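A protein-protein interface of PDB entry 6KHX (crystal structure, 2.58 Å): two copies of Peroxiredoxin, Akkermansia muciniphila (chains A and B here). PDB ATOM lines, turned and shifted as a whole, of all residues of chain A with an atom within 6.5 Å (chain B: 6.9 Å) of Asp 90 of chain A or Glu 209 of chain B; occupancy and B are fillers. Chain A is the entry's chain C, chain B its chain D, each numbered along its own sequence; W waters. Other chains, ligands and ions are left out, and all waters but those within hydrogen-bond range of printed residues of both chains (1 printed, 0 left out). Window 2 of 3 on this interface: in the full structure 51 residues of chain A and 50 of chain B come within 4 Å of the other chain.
Along chain A the printed residues that touch a printed residue of chain B span positions 89 to 93.
The backbone carbonyl oxygen (O) of Ala 202 of chain B sits at hydrogen-bond distance from the side-chain hydroxyl (OG) of Ser 206 of chain B.
O of Pro 88 of chain A sits at hydrogen-bond distance from N of Gly 93 of chain A, at 2.9 Å.
Among the printed residues, merely in contact across the chains: Arg 89 of chain A with Leu 205 of chain B, Arg 89 of chain A with Glu 209 of chain B, Gly 92 of chain A with Leu 205 of chain B and Gly 93 of chain A with Leu 205 of chain B.
No position is printed for both chains.
Of chain B, only Ala 202, Ser 206 and Glu 209 come within 4 Å of Asp 90 of chain A.
Of the printed residues of chain B, Gly 93 of chain A touches Leu 205.
Of the printed residues of chain B, Arg 89 of chain A touches Leu 205 (3.1 Å) and Glu 209 (3.2 Å).
Printed residues of chain A within 4 Å of Leu 205 of chain B: Arg 89, Gly 92 and Gly 93.
Lys 207 of chain B touches none of the printed residues of chain A.
Pro 88 of chain A touches none of the printed residues of chain B.
The nearest residue of chain B that does not touch Asp 90 of chain A is Leu 205 of chain B (4.5 Å).
The nearest residue of chain A that does not touch Glu 209 of chain B is Pro 88 of chain A (5.6 Å).
Water W1 lies within hydrogen-bond range of OE1 of Glu 209 of chain B (3.0 Å) and OD2 of Asp 90 of chain A (3.1 Å).
O of Asp 90 of chain A lies close to O of Ala 202 of chain B.
The backbone carbonyl oxygen (O) of Asp 90 of chain A sits at hydrogen-bond distance from the side-chain hydroxyl (OG) of Ser 206 of chain B, 2.9 Å away.
The side-chain carboxylate (OD2) of Asp 90 of chain A lies close to the side-chain carboxylate (OE1) of Glu 209 of chain B.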
ATOM      1  N   THR A  87      16.857 -19.787 -15.959  1.00  0.00           N
ATOM      2  CA  THR A  87      15.723 -18.960 -16.313  1.00  0.00           C
ATOM      3  C   THR A  87      14.907 -19.679 -17.368  1.00  0.00           C
ATOM      4  O   THR A  87      15.468 -20.107 -18.385  1.00  0.00           O
ATOM      5  CB  THR A  87      16.188 -17.597 -16.849  1.00  0.00           C
ATOM      6  OG1 THR A  87      16.914 -16.900 -15.829  1.00  0.00           O
ATOM      7  CG2 THR A  87      15.006 -16.751 -17.288  1.00  0.00           C
ATOM      8  N   PRO A  88      13.603 -19.847 -17.166  1.00  0.00           N
ATOM      9  CA  PRO A  88      12.803 -20.580 -18.151  1.00  0.00           C
ATOM     10  C   PRO A  88      12.767 -19.855 -19.487  1.00  0.00           C
ATOM     11  O   PRO A  88      12.827 -18.625 -19.556  1.00  0.00           O
ATOM     12  CB  PRO A  88      11.416 -20.657 -17.499  1.00  0.00           C
ATOM     13  CG  PRO A  88      11.402 -19.566 -16.477  1.00  0.00           C
ATOM     14  CD  PRO A  88      12.813 -19.462 -15.982  1.00  0.00           C
ATOM     15  N   ARG A  89      12.687 -20.648 -20.562  1.00  0.00           N
ATOM     16  CA  ARG A  89      12.763 -20.097 -21.913  1.00  0.00           C
ATOM     17  C   ARG A  89      11.616 -19.138 -22.210  1.00  0.00           C
ATOM     18  O   ARG A  89      11.808 -18.136 -22.907  1.00  0.00           O
ATOM     19  CB  ARG A  89      12.787 -21.223 -22.944  1.00  0.00           C
ATOM     20  CG  ARG A  89      13.936 -22.182 -22.771  1.00  0.00           C
ATOM     21  CD  ARG A  89      13.984 -23.194 -23.891  1.00  0.00           C
ATOM     22  NE  ARG A  89      15.108 -24.103 -23.709  1.00  0.00           N
ATOM     23  CZ  ARG A  89      15.424 -25.086 -24.544  1.00  0.00           C
ATOM     24  NH1 ARG A  89      14.699 -25.294 -25.633  1.00  0.00           N
ATOM     25  NH2 ARG A  89      16.467 -25.864 -24.284  1.00  0.00           N
ATOM     26  N   ASP A  90      10.412 -19.421 -21.698  1.00  0.00           N
ATOM     27  CA  ASP A  90       9.293 -18.529 -21.983  1.00  0.00           C
ATOM     28  C   ASP A  90       9.439 -17.165 -21.319  1.00  0.00           C
ATOM     29  O   ASP A  90       8.599 -16.290 -21.554  1.00  0.00           O
ATOM     30  CB  ASP A  90       7.958 -19.171 -21.587  1.00  0.00           C
ATOM     31  CG  ASP A  90       7.951 -19.693 -20.173  1.00  0.00           C
ATOM     32  OD1 ASP A  90       8.045 -18.882 -19.230  1.00  0.00           O
ATOM     33  OD2 ASP A  90       7.800 -20.921 -20.009  1.00  0.00           O
ATOM     34  N   GLN A  91      10.462 -16.967 -20.493  1.00  0.00           N
ATOM     35  CA  GLN A  91      10.784 -15.654 -19.952  1.00  0.00           C
ATOM     36  C   GLN A  91      12.092 -15.109 -20.514  1.00  0.00           C
ATOM     37  O   GLN A  91      12.673 -14.184 -19.941  1.00  0.00           O
ATOM     38  CB  GLN A  91      10.825 -15.683 -18.425  1.00  0.00           C
ATOM     39  CG  GLN A  91       9.492 -16.000 -17.799  1.00  0.00           C
ATOM     40  CD  GLN A  91       9.513 -15.873 -16.291  1.00  0.00           C
ATOM     41  OE1 GLN A  91      10.536 -16.119 -15.644  1.00  0.00           O
ATOM     42  NE2 GLN A  91       8.380 -15.465 -15.720  1.00  0.00           N
ATOM     43  N   GLY A  92      12.565 -15.667 -21.625  1.00  0.00           N
ATOM     44  CA  GLY A  92      13.813 -15.256 -22.230  1.00  0.00           C
ATOM     45  C   GLY A  92      15.039 -16.020 -21.787  1.00  0.00           C
ATOM     46  O   GLY A  92      16.149 -15.655 -22.191  1.00  0.00           O
ATOM     47  N   GLY A  93      14.880 -17.077 -20.991  1.00  0.00           N
ATOM     48  CA  GLY A  93      16.017 -17.818 -20.492  1.00  0.00           C
ATOM     49  C   GLY A  93      16.507 -18.874 -21.463  1.00  0.00           C
ATOM     50  O   GLY A  93      15.943 -19.102 -22.535  1.00  0.00           O
ATOM     51  N   VAL B 201      11.625 -10.930 -26.695  1.00  0.00           N
ATOM     52  CA  VAL B 201      12.295 -12.224 -26.612  1.00  0.00           C
ATOM     53  C   VAL B 201      11.453 -13.211 -25.810  1.00  0.00           C
ATOM     54  O   VAL B 201      11.345 -14.390 -26.177  1.00  0.00           O
ATOM     55  CB  VAL B 201      13.719 -12.065 -26.036  1.00  0.00           C
ATOM     56  CG1 VAL B 201      13.694 -11.444 -24.647  1.00  0.00           C
ATOM     57  CG2 VAL B 201      14.428 -13.401 -26.000  1.00  0.00           C
ATOM     58  N   ALA B 202      10.809 -12.744 -24.731  1.00  0.00           N
ATOM     59  CA  ALA B 202       9.939 -13.634 -23.966  1.00  0.00           C
ATOM     60  C   ALA B 202       8.793 -14.150 -24.828  1.00  0.00           C
ATOM     61  O   ALA B 202       8.463 -15.342 -24.788  1.00  0.00           O
ATOM     62  CB  ALA B 202       9.410 -12.920 -22.723  1.00  0.00           C
ATOM     63  N   SER B 203       8.188 -13.270 -25.633  1.00  0.00           N
ATOM     64  CA  SER B 203       7.080 -13.670 -26.490  1.00  0.00           C
ATOM     65  C   SER B 203       7.541 -14.606 -27.599  1.00  0.00           C
ATOM     66  O   SER B 203       6.863 -15.596 -27.899  1.00  0.00           O
ATOM     67  CB  SER B 203       6.405 -12.432 -27.080  1.00  0.00           C
ATOM     68  OG  SER B 203       5.519 -12.788 -28.131  1.00  0.00           O
ATOM     69  N   TYR B 204       8.680 -14.307 -28.229  1.00  0.00           N
ATOM     70  CA  TYR B 204       9.177 -15.174 -29.292  1.00  0.00           C
ATOM     71  C   TYR B 204       9.467 -16.573 -28.761  1.00  0.00           C
ATOM     72  O   TYR B 204       9.091 -17.575 -29.382  1.00  0.00           O
ATOM     73  CB  TYR B 204      10.429 -14.573 -29.937  1.00  0.00           C
ATOM     74  CG  TYR B 204      10.988 -15.448 -31.035  1.00  0.00           C
ATOM     75  CD1 TYR B 204      10.499 -15.356 -32.330  1.00  0.00           C
ATOM     76  CD2 TYR B 204      11.982 -16.379 -30.777  1.00  0.00           C
ATOM     77  CE1 TYR B 204      10.991 -16.153 -33.339  1.00  0.00           C
ATOM     78  CE2 TYR B 204      12.479 -17.186 -31.783  1.00  0.00           C
ATOM     79  CZ  TYR B 204      11.978 -17.067 -33.062  1.00  0.00           C
ATOM     80  OH  TYR B 204      12.463 -17.863 -34.075  1.00  0.00           O
ATOM     81  N   LEU B 205      10.154 -16.663 -27.615  1.00  0.00           N
ATOM     82  CA  LEU B 205      10.514 -17.971 -27.077  1.00  0.00           C
ATOM     83  C   LEU B 205       9.299 -18.711 -26.524  1.00  0.00           C
ATOM     84  O   LEU B 205       9.256 -19.946 -26.578  1.00  0.00           O
ATOM     85  CB  LEU B 205      11.589 -17.813 -26.003  1.00  0.00           C
ATOM     86  CG  LEU B 205      12.981 -17.443 -26.526  1.00  0.00           C
ATOM     87  CD1 LEU B 205      13.998 -17.369 -25.396  1.00  0.00           C
ATOM     88  CD2 LEU B 205      13.427 -18.439 -27.596  1.00  0.00           C
ATOM     89  N   SER B 206       8.294 -17.980 -26.023  1.00  0.00           N
ATOM     90  CA  SER B 206       7.083 -18.628 -25.529  1.00  0.00           C
ATOM     91  C   SER B 206       6.334 -19.324 -26.655  1.00  0.00           C
ATOM     92  O   SER B 206       5.782 -20.413 -26.462  1.00  0.00           O
ATOM     93  CB  SER B 206       6.174 -17.606 -24.849  1.00  0.00           C
ATOM     94  OG  SER B 206       6.718 -17.161 -23.622  1.00  0.00           O
ATOM     95  N   LYS B 207       6.298 -18.706 -27.838  1.00  0.00           N
ATOM     96  CA  LYS B 207       5.612 -19.304 -28.980  1.00  0.00           C
ATOM     97  C   LYS B 207       6.296 -20.582 -29.444  1.00  0.00           C
ATOM     98  O   LYS B 207       5.641 -21.462 -30.015  1.00  0.00           O
ATOM     99  CB  LYS B 207       5.514 -18.289 -30.112  1.00  0.00           C
ATOM    100  CG  LYS B 207       4.717 -17.077 -29.697  1.00  0.00           C
ATOM    101  CD  LYS B 207       4.690 -16.015 -30.760  1.00  0.00           C
ATOM    102  CE  LYS B 207       3.984 -14.790 -30.222  1.00  0.00           C
ATOM    103  NZ  LYS B 207       2.586 -15.077 -29.794  1.00  0.00           N
ATOM    104  N   LEU B 208       7.609 -20.691 -29.238  1.00  0.00           N
ATOM    105  CA  LEU B 208       8.303 -21.926 -29.579  1.00  0.00           C
ATOM    106  C   LEU B 208       7.838 -23.075 -28.693  1.00  0.00           C
ATOM    107  O   LEU B 208       7.798 -24.227 -29.141  1.00  0.00           O
ATOM    108  CB  LEU B 208       9.813 -21.723 -29.446  1.00  0.00           C
ATOM    109  CG  LEU B 208      10.531 -20.946 -30.552  1.00  0.00           C
ATOM    110  CD1 LEU B 208      12.038 -21.060 -30.394  1.00  0.00           C
ATOM    111  CD2 LEU B 208      10.104 -21.449 -31.920  1.00  0.00           C
ATOM    112  N   GLU B 209       7.470 -22.774 -27.446  1.00  0.00           N
ATOM    113  CA  GLU B 209       6.962 -23.750 -26.488  1.00  0.00           C
ATOM    114  C   GLU B 209       5.445 -23.893 -26.529  1.00  0.00           C
ATOM    115  O   GLU B 209       4.888 -24.687 -25.763  1.00  0.00           O
ATOM    116  CB  GLU B 209       7.397 -23.374 -25.066  1.00  0.00           C
ATOM    117  CG  GLU B 209       8.901 -23.409 -24.852  1.00  0.00           C
ATOM    118  CD  GLU B 209       9.295 -23.138 -23.412  1.00  0.00           C
ATOM    119  OE1 GLU B 209       8.450 -22.635 -22.640  1.00  0.00           O
ATOM    120  OE2 GLU B 209      10.455 -23.435 -23.050  1.00  0.00           O
ATOM    121  N   HIS B 210       4.765 -23.137 -27.390  1.00  0.00           N
ATOM    122  CA  HIS B 210       3.334 -23.292 -27.597  1.00  0.00           C
ATOM    123  C   HIS B 210       3.003 -24.033 -28.886  1.00  0.00           C
ATOM    124  O   HIS B 210       1.924 -24.629 -28.982  1.00  0.00           O
ATOM    125  CB  HIS B 210       2.655 -21.917 -27.611  1.00  0.00           C
ATOM    126  CG  HIS B 210       1.327 -21.886 -26.922  1.00  0.00           C
ATOM    127  ND1 HIS B 210       0.711 -23.020 -26.438  1.00  0.00           N
ATOM    128  CD2 HIS B 210       0.500 -20.855 -26.629  1.00  0.00           C
ATOM    129  CE1 HIS B 210      -0.439 -22.690 -25.880  1.00  0.00           C
ATOM    130  NE2 HIS B 210      -0.592 -21.380 -25.982  1.00  0.00           N
ATOM    131  N   HIS B 211       3.907 -24.013 -29.866  1.00  0.00           N
ATOM    132  CA  HIS B 211       3.704 -24.674 -31.152  1.00  0.00           C
ATOM    133  C   HIS B 211       4.891 -25.569 -31.487  1.00  0.00           C
ATOM    134  O   HIS B 211       5.916 -25.091 -31.976  1.00  0.00           O
ATOM    135  CB  HIS B 211       3.501 -23.644 -32.269  1.00  0.00           C
ATOM    136  CG  HIS B 211       2.411 -22.656 -31.989  1.00  0.00           C
ATOM    137  ND1 HIS B 211       2.538 -21.649 -31.056  1.00  0.00           N
ATOM    138  CD2 HIS B 211       1.172 -22.520 -32.521  1.00  0.00           C
ATOM    139  CE1 HIS B 211       1.425 -20.937 -31.023  1.00  0.00           C
ATOM    140  NE2 HIS B 211       0.581 -21.444 -31.903  1.00  0.00           N
HETATM  141  O   HOH W   1       5.613 -21.927 -22.018  1.00  0.00           O
